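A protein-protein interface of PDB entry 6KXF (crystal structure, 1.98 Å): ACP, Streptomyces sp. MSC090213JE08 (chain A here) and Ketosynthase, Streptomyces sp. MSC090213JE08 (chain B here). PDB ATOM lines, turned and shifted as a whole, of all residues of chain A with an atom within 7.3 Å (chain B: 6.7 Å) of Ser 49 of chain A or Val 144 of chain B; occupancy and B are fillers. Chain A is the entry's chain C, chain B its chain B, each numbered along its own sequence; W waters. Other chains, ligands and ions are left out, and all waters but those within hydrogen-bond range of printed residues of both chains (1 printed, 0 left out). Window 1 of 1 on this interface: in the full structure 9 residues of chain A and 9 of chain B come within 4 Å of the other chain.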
ATOM      1  N   ILE A  15      -9.395 -17.792   8.510  1.00  0.00           N
ATOM      2  CA  ILE A  15      -8.910 -18.673   9.576  1.00  0.00           C
ATOM      3  C   ILE A  15     -10.009 -18.783  10.645  1.00  0.00           C
ATOM      4  O   ILE A  15     -10.479 -19.904  10.912  1.00  0.00           O
ATOM      5  CB  ILE A  15      -7.559 -18.184  10.148  1.00  0.00           C
ATOM      6  CG1 ILE A  15      -6.399 -18.484   9.191  1.00  0.00           C
ATOM      7  CG2 ILE A  15      -7.301 -18.778  11.527  1.00  0.00           C
ATOM      8  CD1 ILE A  15      -5.139 -17.680   9.457  1.00  0.00           C
ATOM      9  N   ASN A  19     -12.684 -21.973  11.961  1.00  0.00           N
ATOM     10  CA  ASN A  19     -12.441 -22.526  13.315  1.00  0.00           C
ATOM     11  C   ASN A  19     -13.648 -22.316  14.245  1.00  0.00           C
ATOM     12  O   ASN A  19     -13.775 -23.055  15.228  1.00  0.00           O
ATOM     13  CB  ASN A  19     -11.162 -21.956  13.931  1.00  0.00           C
ATOM     14  CG  ASN A  19      -9.927 -22.505  13.260  1.00  0.00           C
ATOM     15  OD1 ASN A  19      -9.652 -23.698  13.330  1.00  0.00           O
ATOM     16  ND2 ASN A  19      -9.194 -21.650  12.569  1.00  0.00           N
ATOM     17  N   LYS A  43     -13.237 -23.487  20.600  1.00  0.00           N
ATOM     18  CA  LYS A  43     -13.349 -22.660  19.397  1.00  0.00           C
ATOM     19  C   LYS A  43     -12.207 -21.630  19.405  1.00  0.00           C
ATOM     20  O   LYS A  43     -11.340 -21.672  18.523  1.00  0.00           O
ATOM     21  CB  LYS A  43     -14.751 -22.037  19.312  1.00  0.00           C
ATOM     22  N   LEU A  44     -12.161 -20.796  20.450  1.00  0.00           N
ATOM     23  CA  LEU A  44     -11.177 -19.718  20.578  1.00  0.00           C
ATOM     24  C   LEU A  44      -9.742 -20.256  20.558  1.00  0.00           C
ATOM     25  O   LEU A  44      -8.864 -19.602  20.007  1.00  0.00           O
ATOM     26  CB  LEU A  44     -11.444 -18.902  21.848  1.00  0.00           C
ATOM     27  CG  LEU A  44     -12.243 -17.626  21.591  1.00  0.00           C
ATOM     28  CD1 LEU A  44     -13.545 -17.967  20.865  1.00  0.00           C
ATOM     29  CD2 LEU A  44     -12.504 -16.858  22.881  1.00  0.00           C
ATOM     30  N   ILE A  45      -9.508 -21.442  21.143  1.00  0.00           N
ATOM     31  CA  ILE A  45      -8.168 -22.059  21.128  1.00  0.00           C
ATOM     32  C   ILE A  45      -7.840 -22.484  19.690  1.00  0.00           C
ATOM     33  O   ILE A  45      -6.720 -22.288  19.213  1.00  0.00           O
ATOM     34  CB  ILE A  45      -8.069 -23.223  22.149  1.00  0.00           C
ATOM     35  CG1 ILE A  45      -7.938 -22.693  23.583  1.00  0.00           C
ATOM     36  CG2 ILE A  45      -6.936 -24.174  21.792  1.00  0.00           C
ATOM     37  CD1 ILE A  45      -8.364 -23.677  24.651  1.00  0.00           C
ATOM     38  N   ASP A  46      -8.817 -23.046  18.981  1.00  0.00           N
ATOM     39  CA  ASP A  46      -8.563 -23.468  17.587  1.00  0.00           C
ATOM     40  C   ASP A  46      -8.120 -22.241  16.755  1.00  0.00           C
ATOM     41  O   ASP A  46      -7.218 -22.367  15.905  1.00  0.00           O
ATOM     42  CB  ASP A  46      -9.783 -24.193  16.993  1.00  0.00           C
ATOM     43  CG  ASP A  46      -9.556 -25.619  16.484  1.00  0.00           C
ATOM     44  OD1 ASP A  46      -8.389 -26.003  16.165  1.00  0.00           O
ATOM     45  OD2 ASP A  46     -10.568 -26.345  16.381  1.00  0.00           O
ATOM     46  N   VAL A  47      -8.700 -21.056  17.025  1.00  0.00           N
ATOM     47  CA  VAL A  47      -8.371 -19.829  16.248  1.00  0.00           C
ATOM     48  C   VAL A  47      -6.990 -19.308  16.654  1.00  0.00           C
ATOM     49  O   VAL A  47      -6.190 -19.008  15.774  1.00  0.00           O
ATOM     50  CB  VAL A  47      -9.427 -18.705  16.308  1.00  0.00           C
ATOM     51  CG1 VAL A  47     -10.844 -19.246  16.303  1.00  0.00           C
ATOM     52  CG2 VAL A  47      -9.229 -17.742  17.459  1.00  0.00           C
ATOM     53  N   LEU A  48      -6.697 -19.231  17.957  1.00  0.00           N
ATOM     54  CA  LEU A  48      -5.354 -18.796  18.388  1.00  0.00           C
ATOM     55  C   LEU A  48      -4.296 -19.750  17.796  1.00  0.00           C
ATOM     56  O   LEU A  48      -3.261 -19.288  17.270  1.00  0.00           O
ATOM     57  CB  LEU A  48      -5.304 -18.709  19.919  1.00  0.00           C
ATOM     58  CG  LEU A  48      -3.941 -18.328  20.500  1.00  0.00           C
ATOM     59  CD1 LEU A  48      -4.095 -17.765  21.907  1.00  0.00           C
ATOM     60  CD2 LEU A  48      -2.974 -19.517  20.487  1.00  0.00           C
ATOM     61  N   SER A  49      -4.587 -21.061  17.800  1.00  0.00           N
ATOM     62  CA  SER A  49      -3.656 -22.102  17.291  1.00  0.00           C
ATOM     63  C   SER A  49      -3.415 -21.932  15.787  1.00  0.00           C
ATOM     64  O   SER A  49      -2.279 -22.133  15.317  1.00  0.00           O
ATOM     65  CB  SER A  49      -4.124 -23.514  17.576  1.00  0.00           C
ATOM     66  OG  SER A  49      -3.169 -24.470  17.067  1.00  0.00           O
ATOM     67  N   ALA A  50      -4.490 -21.649  15.040  1.00  0.00           N
ATOM     68  CA  ALA A  50      -4.425 -21.439  13.561  1.00  0.00           C
ATOM     69  C   ALA A  50      -3.602 -20.177  13.224  1.00  0.00           C
ATOM     70  O   ALA A  50      -2.699 -20.232  12.404  1.00  0.00           O
ATOM     71  CB  ALA A  50      -5.822 -21.376  12.971  1.00  0.00           C
ATOM     72  N   LEU A  51      -3.872 -19.058  13.902  1.00  0.00           N
ATOM     73  CA  LEU A  51      -3.092 -17.833  13.690  1.00  0.00           C
ATOM     74  C   LEU A  51      -1.595 -18.099  13.926  1.00  0.00           C
ATOM     75  O   LEU A  51      -0.772 -17.730  13.088  1.00  0.00           O
ATOM     76  CB  LEU A  51      -3.606 -16.726  14.612  1.00  0.00           C
ATOM     77  CG  LEU A  51      -5.084 -16.373  14.459  1.00  0.00           C
ATOM     78  CD1 LEU A  51      -5.501 -15.317  15.472  1.00  0.00           C
ATOM     79  CD2 LEU A  51      -5.388 -15.910  13.039  1.00  0.00           C
ATOM     80  N   GLU A  52      -1.247 -18.735  15.059  1.00  0.00           N
ATOM     81  CA  GLU A  52       0.139 -19.020  15.417  1.00  0.00           C
ATOM     82  C   GLU A  52       0.841 -19.743  14.260  1.00  0.00           C
ATOM     83  O   GLU A  52       1.962 -19.413  13.882  1.00  0.00           O
ATOM     84  CB  GLU A  52       0.212 -19.904  16.669  1.00  0.00           C
ATOM     85  CG  GLU A  52       0.126 -19.172  18.003  1.00  0.00           C
ATOM     86  CD  GLU A  52       0.492 -20.033  19.219  1.00  0.00           C
ATOM     87  OE1 GLU A  52       0.248 -21.252  19.190  1.00  0.00           O
ATOM     88  OE2 GLU A  52       1.044 -19.491  20.188  1.00  0.00           O
ATOM     89  N   MET A  53       0.173 -20.766  13.718  1.00  0.00           N
ATOM     90  CA  MET A  53       0.742 -21.584  12.664  1.00  0.00           C
ATOM     91  C   MET A  53       0.885 -20.774  11.368  1.00  0.00           C
ATOM     92  O   MET A  53       1.914 -20.884  10.698  1.00  0.00           O
ATOM     93  CB  MET A  53      -0.125 -22.811  12.392  1.00  0.00           C
ATOM     94  CG  MET A  53       0.671 -23.983  11.875  1.00  0.00           C
ATOM     95  SD  MET A  53      -0.334 -25.471  11.776  1.00  0.00           S
ATOM     96  CE  MET A  53      -1.256 -25.409  13.320  1.00  0.00           C
ATOM     97  N   GLU A  54      -0.146 -19.982  11.035  1.00  0.00           N
ATOM     98  CA  GLU A  54      -0.184 -19.176   9.814  1.00  0.00           C
ATOM     99  C   GLU A  54       1.082 -18.320   9.717  1.00  0.00           C
ATOM    100  O   GLU A  54       1.735 -18.290   8.678  1.00  0.00           O
ATOM    101  CB  GLU A  54      -1.417 -18.268   9.794  1.00  0.00           C
ATOM    102  CG  GLU A  54      -1.650 -17.547   8.466  1.00  0.00           C
ATOM    103  CD  GLU A  54      -2.038 -18.425   7.285  1.00  0.00           C
ATOM    104  OE1 GLU A  54      -2.060 -17.909   6.156  1.00  0.00           O
ATOM    105  OE2 GLU A  54      -2.316 -19.621   7.490  1.00  0.00           O
ATOM    106  N   ILE A  57       4.089 -17.331  14.627  1.00  0.00           N
ATOM    107  CA  ILE A  57       4.211 -16.472  15.814  1.00  0.00           C
ATOM    108  C   ILE A  57       3.805 -17.266  17.060  1.00  0.00           C
ATOM    109  O   ILE A  57       3.272 -18.393  16.977  1.00  0.00           O
ATOM    110  CB  ILE A  57       3.368 -15.183  15.695  1.00  0.00           C
ATOM    111  CG1 ILE A  57       1.890 -15.486  15.448  1.00  0.00           C
ATOM    112  CG2 ILE A  57       3.944 -14.250  14.639  1.00  0.00           C
ATOM    113  CD1 ILE A  57       0.974 -14.342  15.812  1.00  0.00           C
ATOM    114  N   ILE A  59       1.391 -16.530  20.322  1.00  0.00           N
ATOM    115  CA  ILE A  59       0.413 -15.740  21.041  1.00  0.00           C
ATOM    116  C   ILE A  59       0.272 -16.327  22.449  1.00  0.00           C
ATOM    117  O   ILE A  59       0.071 -17.538  22.613  1.00  0.00           O
ATOM    118  CB  ILE A  59      -0.936 -15.715  20.306  1.00  0.00           C
ATOM    119  CG1 ILE A  59      -0.793 -15.296  18.839  1.00  0.00           C
ATOM    120  CG2 ILE A  59      -1.919 -14.829  21.054  1.00  0.00           C
ATOM    121  CD1 ILE A  59      -2.029 -15.553  17.995  1.00  0.00           C
ATOM    122  N   MET A  61      -1.402 -17.428  25.632  1.00  0.00           N
ATOM    123  CA  MET A  61      -2.772 -17.973  25.748  1.00  0.00           C
ATOM    124  C   MET A  61      -3.529 -17.355  26.934  1.00  0.00           C
ATOM    125  O   MET A  61      -4.732 -17.581  27.079  1.00  0.00           O
ATOM    126  CB  MET A  61      -2.782 -19.507  25.803  1.00  0.00           C
ATOM    127  CG  MET A  61      -2.325 -20.098  24.476  1.00  0.00           C
ATOM    128  SD  MET A  61      -2.453 -21.898  24.311  1.00  0.00           S
ATOM    129  CE  MET A  61      -4.229 -22.070  24.243  1.00  0.00           C
ATOM    130  N   LEU A  64      -6.444 -14.927  25.513  1.00  0.00           N
ATOM    131  CA  LEU A  64      -7.690 -15.534  24.982  1.00  0.00           C
ATOM    132  C   LEU A  64      -8.912 -14.731  25.429  1.00  0.00           C
ATOM    133  O   LEU A  64      -9.827 -14.532  24.629  1.00  0.00           O
ATOM    134  CB  LEU A  64      -7.835 -16.991  25.445  1.00  0.00           C
ATOM    135  CG  LEU A  64      -7.106 -18.047  24.611  1.00  0.00           C
ATOM    136  CD1 LEU A  64      -7.105 -19.383  25.341  1.00  0.00           C
ATOM    137  CD2 LEU A  64      -7.724 -18.194  23.222  1.00  0.00           C
ATOM    138  N   MET A  67      -9.893 -11.931  22.868  1.00  0.00           N
ATOM    139  CA  MET A  67     -10.009 -12.241  21.455  1.00  0.00           C
ATOM    140  C   MET A  67     -11.489 -12.397  21.103  1.00  0.00           C
ATOM    141  O   MET A  67     -11.992 -13.506  20.951  1.00  0.00           O
ATOM    142  CB  MET A  67      -9.235 -13.520  21.134  1.00  0.00           C
ATOM    143  CG  MET A  67      -7.753 -13.296  21.157  1.00  0.00           C
ATOM    144  SD  MET A  67      -6.799 -14.821  20.997  1.00  0.00           S
ATOM    145  CE  MET A  67      -7.327 -15.439  19.400  1.00  0.00           C
ATOM    146  N   ASP B 130      -0.767 -38.280  13.214  1.00  0.00           N
ATOM    147  CA  ASP B 130      -0.912 -36.948  12.551  1.00  0.00           C
ATOM    148  C   ASP B 130      -0.523 -35.826  13.526  1.00  0.00           C
ATOM    149  O   ASP B 130       0.180 -34.893  13.157  1.00  0.00           O
ATOM    150  CB  ASP B 130      -2.341 -36.719  12.040  1.00  0.00           C
ATOM    151  CG  ASP B 130      -2.692 -37.455  10.751  1.00  0.00           C
ATOM    152  OD1 ASP B 130      -1.747 -37.969  10.103  1.00  0.00           O
ATOM    153  OD2 ASP B 130      -3.923 -37.537  10.422  1.00  0.00           O
ATOM    154  N   PHE B 131      -0.975 -35.934  14.786  1.00  0.00           N
ATOM    155  CA  PHE B 131      -0.570 -35.007  15.870  1.00  0.00           C
ATOM    156  C   PHE B 131       0.959 -34.951  15.995  1.00  0.00           C
ATOM    157  O   PHE B 131       1.583 -33.900  15.932  1.00  0.00           O
ATOM    158  CB  PHE B 131      -1.225 -35.464  17.178  1.00  0.00           C
ATOM    159  CG  PHE B 131      -0.925 -34.597  18.372  1.00  0.00           C
ATOM    160  CD1 PHE B 131       0.260 -34.734  19.069  1.00  0.00           C
ATOM    161  CD2 PHE B 131      -1.844 -33.658  18.809  1.00  0.00           C
ATOM    162  CE1 PHE B 131       0.523 -33.937  20.171  1.00  0.00           C
ATOM    163  CE2 PHE B 131      -1.585 -32.870  19.923  1.00  0.00           C
ATOM    164  CZ  PHE B 131      -0.394 -32.997  20.588  1.00  0.00           C
ATOM    165  N   LEU B 132       1.588 -36.108  16.178  1.00  0.00           N
ATOM    166  CA  LEU B 132       3.019 -36.168  16.405  1.00  0.00           C
ATOM    167  C   LEU B 132       3.787 -35.720  15.147  1.00  0.00           C
ATOM    168  O   LEU B 132       4.844 -35.059  15.264  1.00  0.00           O
ATOM    169  CB  LEU B 132       3.419 -37.584  16.825  1.00  0.00           C
ATOM    170  CG  LEU B 132       3.077 -37.950  18.268  1.00  0.00           C
ATOM    171  CD1 LEU B 132       3.230 -39.431  18.505  1.00  0.00           C
ATOM    172  CD2 LEU B 132       3.929 -37.160  19.239  1.00  0.00           C
ATOM    173  N   GLN B 134       2.919 -33.524  13.018  1.00  0.00           N
ATOM    174  CA  GLN B 134       2.964 -32.081  12.898  1.00  0.00           C
ATOM    175  C   GLN B 134       3.846 -31.497  14.015  1.00  0.00           C
ATOM    176  O   GLN B 134       4.575 -30.505  13.763  1.00  0.00           O
ATOM    177  CB  GLN B 134       1.565 -31.497  12.638  1.00  0.00           C
ATOM    178  CG  GLN B 134       0.550 -31.607  13.746  1.00  0.00           C
ATOM    179  CD  GLN B 134      -0.847 -31.220  13.294  1.00  0.00           C
ATOM    180  OE1 GLN B 134      -1.839 -31.737  13.797  1.00  0.00           O
ATOM    181  NE2 GLN B 134      -0.964 -30.276  12.372  1.00  0.00           N
ATOM    182  N   SER B 135       3.895 -32.147  15.190  1.00  0.00           N
ATOM    183  CA  SER B 135       4.793 -31.698  16.266  1.00  0.00           C
ATOM    184  C   SER B 135       6.248 -31.723  15.800  1.00  0.00           C
ATOM    185  O   SER B 135       7.022 -30.867  16.173  1.00  0.00           O
ATOM    186  CB  SER B 135       4.678 -32.533  17.527  1.00  0.00           C
ATOM    187  OG  SER B 135       5.577 -32.024  18.496  1.00  0.00           O
ATOM    188  N   TYR B 136       6.614 -32.778  15.069  1.00  0.00           N
ATOM    189  CA  TYR B 136       7.982 -32.991  14.616  1.00  0.00           C
ATOM    190  C   TYR B 136       8.346 -32.125  13.391  1.00  0.00           C
ATOM    191  O   TYR B 136       9.527 -31.838  13.199  1.00  0.00           O
ATOM    192  CB  TYR B 136       8.205 -34.460  14.253  1.00  0.00           C
ATOM    193  CG  TYR B 136       8.569 -35.336  15.419  1.00  0.00           C
ATOM    194  CD1 TYR B 136       9.779 -35.171  16.074  1.00  0.00           C
ATOM    195  CD2 TYR B 136       7.705 -36.308  15.888  1.00  0.00           C
ATOM    196  CE1 TYR B 136      10.138 -35.974  17.143  1.00  0.00           C
ATOM    197  CE2 TYR B 136       8.043 -37.115  16.966  1.00  0.00           C
ATOM    198  CZ  TYR B 136       9.260 -36.943  17.602  1.00  0.00           C
ATOM    199  OH  TYR B 136       9.623 -37.742  18.647  1.00  0.00           O
ATOM    200  N   ASN B 138       6.335 -29.270  11.924  1.00  0.00           N
ATOM    201  CA  ASN B 138       5.945 -27.872  11.832  1.00  0.00           C
ATOM    202  C   ASN B 138       7.020 -27.033  12.525  1.00  0.00           C
ATOM    203  O   ASN B 138       7.989 -27.580  13.018  1.00  0.00           O
ATOM    204  CB  ASN B 138       4.538 -27.627  12.368  1.00  0.00           C
ATOM    205  CG  ASN B 138       3.473 -28.108  11.428  1.00  0.00           C
ATOM    206  OD1 ASN B 138       3.754 -28.381  10.261  1.00  0.00           O
ATOM    207  ND2 ASN B 138       2.255 -28.210  11.930  1.00  0.00           N
ATOM    208  N   ARG B 140       7.095 -24.961  15.107  1.00  0.00           N
ATOM    209  CA  ARG B 140       7.205 -25.092  16.568  1.00  0.00           C
ATOM    210  C   ARG B 140       6.517 -26.390  16.944  1.00  0.00           C
ATOM    211  O   ARG B 140       5.517 -26.732  16.324  1.00  0.00           O
ATOM    212  CB  ARG B 140       6.570 -23.911  17.311  1.00  0.00           C
ATOM    213  CG  ARG B 140       7.303 -22.591  17.107  1.00  0.00           C
ATOM    214  CD  ARG B 140       6.578 -21.451  17.789  1.00  0.00           C
ATOM    215  NE  ARG B 140       6.776 -20.178  17.113  1.00  0.00           N
ATOM    216  CZ  ARG B 140       7.885 -19.465  17.202  1.00  0.00           C
ATOM    217  NH1 ARG B 140       8.872 -19.889  17.975  1.00  0.00           N
ATOM    218  NH2 ARG B 140       8.007 -18.348  16.511  1.00  0.00           N
ATOM    219  N   PRO B 141       7.029 -27.138  17.944  1.00  0.00           N
ATOM    220  CA  PRO B 141       6.562 -28.502  18.176  1.00  0.00           C
ATOM    221  C   PRO B 141       5.180 -28.570  18.855  1.00  0.00           C
ATOM    222  O   PRO B 141       4.650 -29.667  19.019  1.00  0.00           O
ATOM    223  CB  PRO B 141       7.731 -29.096  18.981  1.00  0.00           C
ATOM    224  CG  PRO B 141       8.280 -27.939  19.776  1.00  0.00           C
ATOM    225  CD  PRO B 141       8.064 -26.718  18.905  1.00  0.00           C
ATOM    226  N   PHE B 142       4.596 -27.410  19.195  1.00  0.00           N
ATOM    227  CA  PHE B 142       3.248 -27.310  19.706  1.00  0.00           C
ATOM    228  C   PHE B 142       2.277 -26.748  18.649  1.00  0.00           C
ATOM    229  O   PHE B 142       1.072 -26.510  18.954  1.00  0.00           O
ATOM    230  CB  PHE B 142       3.208 -26.523  21.023  1.00  0.00           C
ATOM    231  CG  PHE B 142       3.624 -25.076  20.958  1.00  0.00           C
ATOM    232  CD1 PHE B 142       4.924 -24.712  21.238  1.00  0.00           C
ATOM    233  CD2 PHE B 142       2.697 -24.083  20.692  1.00  0.00           C
ATOM    234  CE1 PHE B 142       5.317 -23.389  21.169  1.00  0.00           C
ATOM    235  CE2 PHE B 142       3.086 -22.752  20.641  1.00  0.00           C
ATOM    236  CZ  PHE B 142       4.397 -22.410  20.870  1.00  0.00           C
ATOM    237  N   TYR B 143       2.756 -26.564  17.411  1.00  0.00           N
ATOM    238  CA  TYR B 143       1.864 -26.298  16.254  1.00  0.00           C
ATOM    239  C   TYR B 143       1.180 -27.597  15.840  1.00  0.00           C
ATOM    240  O   TYR B 143       1.571 -28.220  14.852  1.00  0.00           O
ATOM    241  CB  TYR B 143       2.615 -25.684  15.073  1.00  0.00           C
ATOM    242  CG  TYR B 143       3.092 -24.268  15.278  1.00  0.00           C
ATOM    243  CD1 TYR B 143       2.770 -23.547  16.418  1.00  0.00           C
ATOM    244  CD2 TYR B 143       3.846 -23.630  14.300  1.00  0.00           C
ATOM    245  CE1 TYR B 143       3.219 -22.250  16.595  1.00  0.00           C
ATOM    246  CE2 TYR B 143       4.293 -22.328  14.462  1.00  0.00           C
ATOM    247  CZ  TYR B 143       3.975 -21.632  15.614  1.00  0.00           C
ATOM    248  OH  TYR B 143       4.405 -20.343  15.795  1.00  0.00           O
ATOM    249  N   VAL B 144       0.163 -27.973  16.623  1.00  0.00           N
ATOM    250  CA  VAL B 144      -0.631 -29.158  16.403  1.00  0.00           C
ATOM    251  C   VAL B 144      -2.100 -28.743  16.284  1.00  0.00           C
ATOM    252  O   VAL B 144      -2.500 -27.664  16.743  1.00  0.00           O
ATOM    253  CB  VAL B 144      -0.399 -30.207  17.517  1.00  0.00           C
ATOM    254  CG1 VAL B 144       1.068 -30.596  17.586  1.00  0.00           C
ATOM    255  CG2 VAL B 144      -0.892 -29.737  18.874  1.00  0.00           C
ATOM    256  N   ASP B 145      -2.891 -29.621  15.662  1.00  0.00           N
ATOM    257  CA  ASP B 145      -4.260 -29.340  15.333  1.00  0.00           C
ATOM    258  C   ASP B 145      -5.079 -29.505  16.607  1.00  0.00           C
ATOM    259  O   ASP B 145      -5.373 -30.636  17.002  1.00  0.00           O
ATOM    260  CB  ASP B 145      -4.754 -30.267  14.217  1.00  0.00           C
ATOM    261  CG  ASP B 145      -6.145 -29.931  13.682  1.00  0.00           C
ATOM    262  OD1 ASP B 145      -6.968 -29.390  14.460  1.00  0.00           O
ATOM    263  OD2 ASP B 145      -6.397 -30.218  12.487  1.00  0.00           O
ATOM    264  N   ALA B 146      -5.459 -28.378  17.216  1.00  0.00           N
ATOM    265  CA  ALA B 146      -6.106 -28.348  18.530  1.00  0.00           C
ATOM    266  C   ALA B 146      -7.490 -28.987  18.483  1.00  0.00           C
ATOM    267  O   ALA B 146      -7.927 -29.620  19.462  1.00  0.00           O
ATOM    268  CB  ALA B 146      -6.175 -26.924  19.043  1.00  0.00           C
ATOM    269  N   GLY B 147      -8.184 -28.835  17.350  1.00  0.00           N
ATOM    270  CA  GLY B 147      -9.528 -29.346  17.214  1.00  0.00           C
ATOM    271  C   GLY B 147      -9.560 -30.861  17.109  1.00  0.00           C
ATOM    272  O   GLY B 147     -10.605 -31.489  17.328  1.00  0.00           O
ATOM    273  N   ILE B 149      -7.533 -32.813  18.946  1.00  0.00           N
ATOM    274  CA  ILE B 149      -7.023 -33.352  20.213  1.00  0.00           C
ATOM    275  C   ILE B 149      -8.082 -34.185  20.921  1.00  0.00           C
ATOM    276  O   ILE B 149      -7.783 -35.295  21.335  1.00  0.00           O
ATOM    277  CB  ILE B 149      -6.425 -32.244  21.100  1.00  0.00           C
ATOM    278  CG1 ILE B 149      -5.039 -31.868  20.575  1.00  0.00           C
ATOM    279  CG2 ILE B 149      -6.394 -32.660  22.570  1.00  0.00           C
ATOM    280  CD1 ILE B 149      -4.573 -30.479  20.975  1.00  0.00           C
HETATM  281  O   HOH W   1      -5.476 -25.824  15.918  1.00  0.00           O
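The side-chain amide nitrogen (ND2) of Asn 138 of chain B lies within hydrogen-bond range of the backbone carbonyl oxygen (O) of Tyr 143 of chain B (3.0 Å).
The guanidinium group (NE) of Arg 140 of chain B is in hydrogen-bond range of the side-chain hydroxyl (OH) of Tyr 143 of chain B (2.7 Å).
The backbone NH (N) of Gly 147 of chain B lies within hydrogen-bond range of the side-chain carboxylate (OD1) of Asp 145 of chain B, at 3.2 Å.
The backbone carbonyl oxygen of Glu 52 of chain A sits at hydrogen-bond distance from the backbone NH of Ile 57 of chain A.
The side-chain carboxylate (OE2) of Glu 52 of chain A sits at hydrogen-bond distance from the backbone NH (N) of Ile 59 of chain A, 3.0 Å away.
The side-chain amide nitrogen of Asn 138 of chain B sits at hydrogen-bond distance from the side-chain sulfur of Met 53 of chain A.
The side-chain hydroxyl of Tyr 143 of chain B is in hydrogen-bond range of the backbone carbonyl oxygen of Glu 52 of chain A (3.2 Å).
OH of Tyr 143 of chain B sits at hydrogen-bond distance from O of Ile 57 of chain A, 2.5 Å away.
OG of Ser 49 of chain A is in hydrogen-bond range of O of Val 144 of chain B (3.3 Å).
N of Gly 147 of chain B sits at hydrogen-bond distance from OD1 of Asp 46 of chain A (3.1 Å).
Water W1 lies within hydrogen-bond range of N of Ala 146 of chain B (2.9 Å), OG of Ser 49 of chain A (2.9 Å) and OD1 of Asp 46 of chain A (2.9 Å).
Printed residues of chain A that touch a printed residue of chain B: Ile 45, Asp 46, Ser 49, Glu 52, Met 53 and Ile 57.
Hydrophobic or aromatic side chains of chain A within 4 Å of the printed part of chain B: Ile 45 and Met 53.
Among the printed residues, 9 pairs touch across the chains.
Among the printed residues, no Asp or Glu carboxylate lies within 4 Å of a Lys or Arg side-chain nitrogen of the other chain.
Of chain B, only Val 144 (3.3 Å) comes within 4 Å of Ser 49 of chain A.
Val 144 of chain B touches just one residue of chain A: Ser 49 (3.3 Å).
Of the printed residues of chain A, Tyr 143 of chain B touches Glu 52 (3.2 Å) and Ile 57 (2.5 Å).
Printed residues of chain A within 4 Å of Asn 138 of chain B: Met 53 (3.8 Å).
Of the printed residues of chain B, Glu 52 of chain A touches Phe 142 and Tyr 143.
The nearest residue of chain B that does not touch Ser 49 of chain A is Ala 146 of chain B (4.2 Å).
The nearest printed residue of chain A that does not touch Phe 142 of chain B is Ser 49 of chain A (5.1 Å).
Among the printed residues, merely in contact across the chains: Ile 45 of chain A with Ala 146 of chain B, Asp 46 of chain A with Ala 146 of chain B, Glu 52 of chain A with Phe 142 of chain B and Ile 57 of chain A with Arg 140 of chain B.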
